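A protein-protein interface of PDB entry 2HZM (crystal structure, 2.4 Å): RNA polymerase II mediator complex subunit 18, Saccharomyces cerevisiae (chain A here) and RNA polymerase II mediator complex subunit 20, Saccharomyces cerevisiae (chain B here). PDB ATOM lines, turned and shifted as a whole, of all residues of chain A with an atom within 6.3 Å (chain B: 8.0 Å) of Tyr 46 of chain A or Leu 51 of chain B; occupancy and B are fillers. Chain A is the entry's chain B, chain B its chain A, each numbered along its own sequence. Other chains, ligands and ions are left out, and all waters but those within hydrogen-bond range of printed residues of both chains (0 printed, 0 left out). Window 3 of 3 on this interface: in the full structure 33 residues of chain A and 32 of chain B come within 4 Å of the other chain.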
ATOM      1  N   PRO A  42      22.251 -23.203   1.859  1.00  0.00           N
ATOM      2  CA  PRO A  42      22.859 -23.232   3.195  1.00  0.00           C
ATOM      3  C   PRO A  42      24.070 -24.154   3.135  1.00  0.00           C
ATOM      4  O   PRO A  42      24.019 -25.186   2.479  1.00  0.00           O
ATOM      5  CB  PRO A  42      21.757 -23.819   4.060  1.00  0.00           C
ATOM      6  CG  PRO A  42      20.503 -23.366   3.355  1.00  0.00           C
ATOM      7  CD  PRO A  42      20.837 -23.617   1.916  1.00  0.00           C
ATOM      8  N   ASN A  43      25.156 -23.765   3.792  1.00  0.00           N
ATOM      9  CA  ASN A  43      26.381 -24.556   3.825  1.00  0.00           C
ATOM     10  C   ASN A  43      26.055 -25.940   4.381  1.00  0.00           C
ATOM     11  O   ASN A  43      25.631 -26.059   5.528  1.00  0.00           O
ATOM     12  CB  ASN A  43      27.406 -23.881   4.734  1.00  0.00           C
ATOM     13  CG  ASN A  43      28.790 -24.475   4.586  1.00  0.00           C
ATOM     14  OD1 ASN A  43      28.938 -25.689   4.367  1.00  0.00           O
ATOM     15  ND2 ASN A  43      29.816 -23.630   4.704  1.00  0.00           N
ATOM     16  N   PRO A  44      26.240 -27.002   3.572  1.00  0.00           N
ATOM     17  CA  PRO A  44      25.954 -28.376   3.995  1.00  0.00           C
ATOM     18  C   PRO A  44      26.800 -28.782   5.177  1.00  0.00           C
ATOM     19  O   PRO A  44      26.387 -29.597   5.992  1.00  0.00           O
ATOM     20  CB  PRO A  44      26.257 -29.197   2.743  1.00  0.00           C
ATOM     21  CG  PRO A  44      27.352 -28.420   2.092  1.00  0.00           C
ATOM     22  CD  PRO A  44      26.830 -26.993   2.221  1.00  0.00           C
ATOM     23  N   SER A  45      27.987 -28.202   5.265  1.00  0.00           N
ATOM     24  CA  SER A  45      28.891 -28.471   6.368  1.00  0.00           C
ATOM     25  C   SER A  45      28.292 -28.024   7.712  1.00  0.00           C
ATOM     26  O   SER A  45      28.724 -28.495   8.762  1.00  0.00           O
ATOM     27  CB  SER A  45      30.227 -27.760   6.125  1.00  0.00           C
ATOM     28  OG  SER A  45      30.961 -27.596   7.329  1.00  0.00           O
ATOM     29  N   TYR A  46      27.297 -27.130   7.684  1.00  0.00           N
ATOM     30  CA  TYR A  46      26.666 -26.648   8.921  1.00  0.00           C
ATOM     31  C   TYR A  46      25.433 -27.451   9.338  1.00  0.00           C
ATOM     32  O   TYR A  46      24.924 -27.284  10.446  1.00  0.00           O
ATOM     33  CB  TYR A  46      26.278 -25.168   8.809  1.00  0.00           C
ATOM     34  CG  TYR A  46      27.430 -24.233   8.510  1.00  0.00           C
ATOM     35  CD1 TYR A  46      28.735 -24.559   8.877  1.00  0.00           C
ATOM     36  CD2 TYR A  46      27.213 -23.002   7.894  1.00  0.00           C
ATOM     37  CE1 TYR A  46      29.795 -23.688   8.637  1.00  0.00           C
ATOM     38  CE2 TYR A  46      28.270 -22.119   7.651  1.00  0.00           C
ATOM     39  CZ  TYR A  46      29.557 -22.469   8.026  1.00  0.00           C
ATOM     40  OH  TYR A  46      30.610 -21.603   7.800  1.00  0.00           O
ATOM     41  N   ASP A  47      24.950 -28.316   8.451  1.00  0.00           N
ATOM     42  CA  ASP A  47      23.789 -29.160   8.747  1.00  0.00           C
ATOM     43  C   ASP A  47      22.610 -28.408   9.353  1.00  0.00           C
ATOM     44  O   ASP A  47      22.465 -28.354  10.577  1.00  0.00           O
ATOM     45  CB  ASP A  47      24.183 -30.280   9.717  1.00  0.00           C
ATOM     46  CG  ASP A  47      25.435 -31.015   9.290  1.00  0.00           C
ATOM     47  OD1 ASP A  47      25.392 -31.744   8.272  1.00  0.00           O
ATOM     48  OD2 ASP A  47      26.470 -30.857   9.974  1.00  0.00           O
ATOM     49  N   VAL A  48      21.766 -27.834   8.506  1.00  0.00           N
ATOM     50  CA  VAL A  48      20.587 -27.119   8.982  1.00  0.00           C
ATOM     51  C   VAL A  48      19.378 -27.637   8.216  1.00  0.00           C
ATOM     52  O   VAL A  48      19.314 -27.512   6.998  1.00  0.00           O
ATOM     53  CB  VAL A  48      20.711 -25.595   8.766  1.00  0.00           C
ATOM     54  CG1 VAL A  48      19.441 -24.906   9.244  1.00  0.00           C
ATOM     55  CG2 VAL A  48      21.917 -25.057   9.525  1.00  0.00           C
ATOM     56  N   ASN A 204      28.501 -16.149   2.294  1.00  0.00           N
ATOM     57  CA  ASN A 204      29.151 -17.102   3.208  1.00  0.00           C
ATOM     58  C   ASN A 204      28.846 -16.600   4.638  1.00  0.00           C
ATOM     59  O   ASN A 204      28.524 -17.386   5.534  1.00  0.00           O
ATOM     60  CB  ASN A 204      30.671 -17.131   2.987  1.00  0.00           C
ATOM     61  CG  ASN A 204      31.087 -17.756   1.649  1.00  0.00           C
ATOM     62  OD1 ASN A 204      32.263 -17.677   1.274  1.00  0.00           O
ATOM     63  ND2 ASN A 204      30.141 -18.380   0.930  1.00  0.00           N
ATOM     64  N   LEU A 206      26.279 -15.246   5.730  1.00  0.00           N
ATOM     65  CA  LEU A 206      24.927 -15.611   6.130  1.00  0.00           C
ATOM     66  C   LEU A 206      24.760 -17.113   6.287  1.00  0.00           C
ATOM     67  O   LEU A 206      23.696 -17.571   6.692  1.00  0.00           O
ATOM     68  CB  LEU A 206      23.909 -15.120   5.107  1.00  0.00           C
ATOM     69  CG  LEU A 206      23.738 -13.613   4.930  1.00  0.00           C
ATOM     70  CD1 LEU A 206      22.738 -13.356   3.802  1.00  0.00           C
ATOM     71  CD2 LEU A 206      23.272 -12.984   6.240  1.00  0.00           C
ATOM     72  N   GLY A 207      25.803 -17.875   5.953  1.00  0.00           N
ATOM     73  CA  GLY A 207      25.738 -19.325   6.082  1.00  0.00           C
ATOM     74  C   GLY A 207      25.393 -20.030   4.779  1.00  0.00           C
ATOM     75  O   GLY A 207      24.946 -21.183   4.785  1.00  0.00           O
ATOM     76  N   TYR A 208      25.609 -19.347   3.657  1.00  0.00           N
ATOM     77  CA  TYR A 208      25.290 -19.910   2.351  1.00  0.00           C
ATOM     78  C   TYR A 208      26.501 -20.124   1.463  1.00  0.00           C
ATOM     79  O   TYR A 208      27.502 -19.435   1.605  1.00  0.00           O
ATOM     80  CB  TYR A 208      24.291 -19.001   1.614  1.00  0.00           C
ATOM     81  CG  TYR A 208      22.872 -19.226   2.034  1.00  0.00           C
ATOM     82  CD1 TYR A 208      22.459 -18.966   3.345  1.00  0.00           C
ATOM     83  CD2 TYR A 208      21.948 -19.772   1.143  1.00  0.00           C
ATOM     84  CE1 TYR A 208      21.161 -19.257   3.756  1.00  0.00           C
ATOM     85  CE2 TYR A 208      20.659 -20.063   1.535  1.00  0.00           C
ATOM     86  CZ  TYR A 208      20.274 -19.805   2.845  1.00  0.00           C
ATOM     87  OH  TYR A 208      18.999 -20.117   3.237  1.00  0.00           O
ATOM     88  N   CYS B  46      23.560 -16.520  15.589  1.00  0.00           N
ATOM     89  CA  CYS B  46      23.596 -17.672  14.690  1.00  0.00           C
ATOM     90  C   CYS B  46      23.449 -18.967  15.503  1.00  0.00           C
ATOM     91  O   CYS B  46      24.075 -19.111  16.557  1.00  0.00           O
ATOM     92  CB  CYS B  46      24.929 -17.666  13.933  1.00  0.00           C
ATOM     93  SG  CYS B  46      25.192 -19.008  12.771  1.00  0.00           S
ATOM     94  N   SER B  47      22.621 -19.890  15.009  1.00  0.00           N
ATOM     95  CA  SER B  47      22.362 -21.184  15.657  1.00  0.00           C
ATOM     96  C   SER B  47      23.423 -22.242  15.359  1.00  0.00           C
ATOM     97  O   SER B  47      23.604 -23.180  16.131  1.00  0.00           O
ATOM     98  CB  SER B  47      21.011 -21.747  15.213  1.00  0.00           C
ATOM     99  OG  SER B  47      19.959 -20.819  15.416  1.00  0.00           O
ATOM    100  N   ILE B  48      24.107 -22.105  14.228  1.00  0.00           N
ATOM    101  CA  ILE B  48      25.137 -23.065  13.837  1.00  0.00           C
ATOM    102  C   ILE B  48      26.108 -23.368  14.980  1.00  0.00           C
ATOM    103  O   ILE B  48      26.508 -22.474  15.725  1.00  0.00           O
ATOM    104  CB  ILE B  48      25.911 -22.552  12.595  1.00  0.00           C
ATOM    105  CG1 ILE B  48      25.116 -22.862  11.327  1.00  0.00           C
ATOM    106  CG2 ILE B  48      27.287 -23.185  12.511  1.00  0.00           C
ATOM    107  CD1 ILE B  48      23.756 -22.222  11.267  1.00  0.00           C
ATOM    108  N   LYS B  49      26.473 -24.639  15.117  1.00  0.00           N
ATOM    109  CA  LYS B  49      27.393 -25.070  16.165  1.00  0.00           C
ATOM    110  C   LYS B  49      28.854 -24.783  15.819  1.00  0.00           C
ATOM    111  O   LYS B  49      29.552 -25.627  15.252  1.00  0.00           O
ATOM    112  CB  LYS B  49      27.224 -26.563  16.439  1.00  0.00           C
ATOM    113  CG  LYS B  49      25.874 -26.952  17.022  1.00  0.00           C
ATOM    114  CD  LYS B  49      25.843 -28.447  17.348  1.00  0.00           C
ATOM    115  CE  LYS B  49      26.951 -28.831  18.340  1.00  0.00           C
ATOM    116  NZ  LYS B  49      27.017 -30.299  18.613  1.00  0.00           N
ATOM    117  N   ASN B  50      29.297 -23.581  16.177  1.00  0.00           N
ATOM    118  CA  ASN B  50      30.662 -23.116  15.938  1.00  0.00           C
ATOM    119  C   ASN B  50      31.179 -23.435  14.535  1.00  0.00           C
ATOM    120  O   ASN B  50      30.466 -24.015  13.716  1.00  0.00           O
ATOM    121  CB  ASN B  50      31.618 -23.711  16.979  1.00  0.00           C
ATOM    122  CG  ASN B  50      32.891 -22.894  17.130  1.00  0.00           C
ATOM    123  OD1 ASN B  50      32.876 -21.794  17.685  1.00  0.00           O
ATOM    124  ND2 ASN B  50      34.000 -23.423  16.625  1.00  0.00           N
ATOM    125  N   LEU B  51      32.426 -23.043  14.278  1.00  0.00           N
ATOM    126  CA  LEU B  51      33.082 -23.267  12.995  1.00  0.00           C
ATOM    127  C   LEU B  51      34.193 -22.238  12.802  1.00  0.00           C
ATOM    128  O   LEU B  51      34.393 -21.359  13.644  1.00  0.00           O
ATOM    129  CB  LEU B  51      32.069 -23.159  11.849  1.00  0.00           C
ATOM    130  CG  LEU B  51      32.501 -23.546  10.428  1.00  0.00           C
ATOM    131  CD1 LEU B  51      33.296 -22.409   9.796  1.00  0.00           C
ATOM    132  CD2 LEU B  51      33.303 -24.849  10.462  1.00  0.00           C
ATOM    133  N   SER B  56      32.363 -15.118  14.740  1.00  0.00           N
ATOM    134  CA  SER B  56      31.294 -14.416  15.438  1.00  0.00           C
ATOM    135  C   SER B  56      29.936 -14.973  15.056  1.00  0.00           C
ATOM    136  O   SER B  56      29.642 -15.162  13.873  1.00  0.00           O
ATOM    137  CB  SER B  56      31.326 -12.923  15.099  1.00  0.00           C
ATOM    138  OG  SER B  56      30.269 -12.226  15.745  1.00  0.00           O
ATOM    139  N   LYS B  57      29.104 -15.234  16.058  1.00  0.00           N
ATOM    140  CA  LYS B  57      27.767 -15.743  15.788  1.00  0.00           C
ATOM    141  C   LYS B  57      26.731 -14.633  15.962  1.00  0.00           C
ATOM    142  O   LYS B  57      25.529 -14.885  16.043  1.00  0.00           O
ATOM    143  CB  LYS B  57      27.445 -16.937  16.696  1.00  0.00           C
ATOM    144  CG  LYS B  57      27.806 -16.758  18.155  1.00  0.00           C
ATOM    145  CD  LYS B  57      27.007 -17.729  19.049  1.00  0.00           C
ATOM    146  CE  LYS B  57      27.210 -19.207  18.673  1.00  0.00           C
ATOM    147  NZ  LYS B  57      28.630 -19.662  18.850  1.00  0.00           N
ATOM    148  N   ASN B 116      16.293 -20.588  10.830  1.00  0.00           N
ATOM    149  CA  ASN B 116      16.957 -21.832  11.186  1.00  0.00           C
ATOM    150  C   ASN B 116      18.440 -21.549  11.363  1.00  0.00           C
ATOM    151  O   ASN B 116      19.182 -22.377  11.886  1.00  0.00           O
ATOM    152  CB  ASN B 116      16.794 -22.861  10.065  1.00  0.00           C
ATOM    153  CG  ASN B 116      17.094 -22.266   8.693  1.00  0.00           C
ATOM    154  OD1 ASN B 116      16.276 -21.527   8.134  1.00  0.00           O
ATOM    155  ND2 ASN B 116      18.270 -22.569   8.155  1.00  0.00           N
ATOM    156  N   ILE B 117      18.879 -20.385  10.902  1.00  0.00           N
ATOM    157  CA  ILE B 117      20.290 -20.017  10.993  1.00  0.00           C
ATOM    158  C   ILE B 117      20.461 -18.795  11.873  1.00  0.00           C
ATOM    159  O   ILE B 117      21.396 -18.699  12.662  1.00  0.00           O
ATOM    160  CB  ILE B 117      20.881 -19.662   9.589  1.00  0.00           C
ATOM    161  CG1 ILE B 117      20.883 -20.892   8.680  1.00  0.00           C
ATOM    162  CG2 ILE B 117      22.315 -19.143   9.723  1.00  0.00           C
ATOM    163  CD1 ILE B 117      21.322 -20.583   7.268  1.00  0.00           C
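Among the printed residues, pairs that only touch across the chains: Val 48 of chain A with Asn 116 of chain B (2.8 Å), Tyr 46 of chain A with Leu 51 of chain B (3.2 Å), Tyr 46 of chain A with Ile 48 of chain B (3.6 Å), Leu 206 of chain A with Ile 117 of chain B (3.7 Å), Tyr 208 of chain A with Ile 117 of chain B (3.8 Å) and Val 48 of chain A with Ile 48 of chain B (3.8 Å).
The side-chain sulfur of Cys 46 of chain B sits close to the backbone NH of Ile 48 of chain B. The backbone NH (N) of Ser 47 of chain B sits at hydrogen-bond distance from the backbone carbonyl oxygen (O) of Ile 117 of chain B, at 2.9 Å. The side-chain amide nitrogen (ND2) of Asn 204 of chain A is in hydrogen-bond range of the backbone carbonyl oxygen (O) of Tyr 208 of chain A (2.9 Å).
Printed residues of chain A that touch a printed residue of chain B: Tyr 46, Val 48, Leu 206 and Tyr 208. Of the 10 printed residues of chain B, 4 touch a printed residue of chain A. Hydrophobic or aromatic side chains of chain B that line the printed part of chain A: Ile 48, Leu 51 and Ile 117. Among the printed residues, 6 pairs touch across the chains.
Of chain B, only Ile 48 and Leu 51 come within 4 Å of Tyr 46 of chain A. Printed residues of chain A within 4 Å of Ile 48 of chain B: Tyr 46 (3.6 Å) and Val 48 (3.8 Å). Lys 49 of chain B touches none of the printed residues of chain A. Asn 50 of chain B touches none of the printed residues of chain A. Leu 51 of chain B touches just one residue of chain A: Tyr 46. Of the printed residues of chain A, Ile 117 of chain B touches Leu 206 (3.7 Å) and Tyr 208 (3.8 Å). The nearest residue of chain B that does not touch Tyr 46 of chain A is Asn 50 of chain B (5.1 Å).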
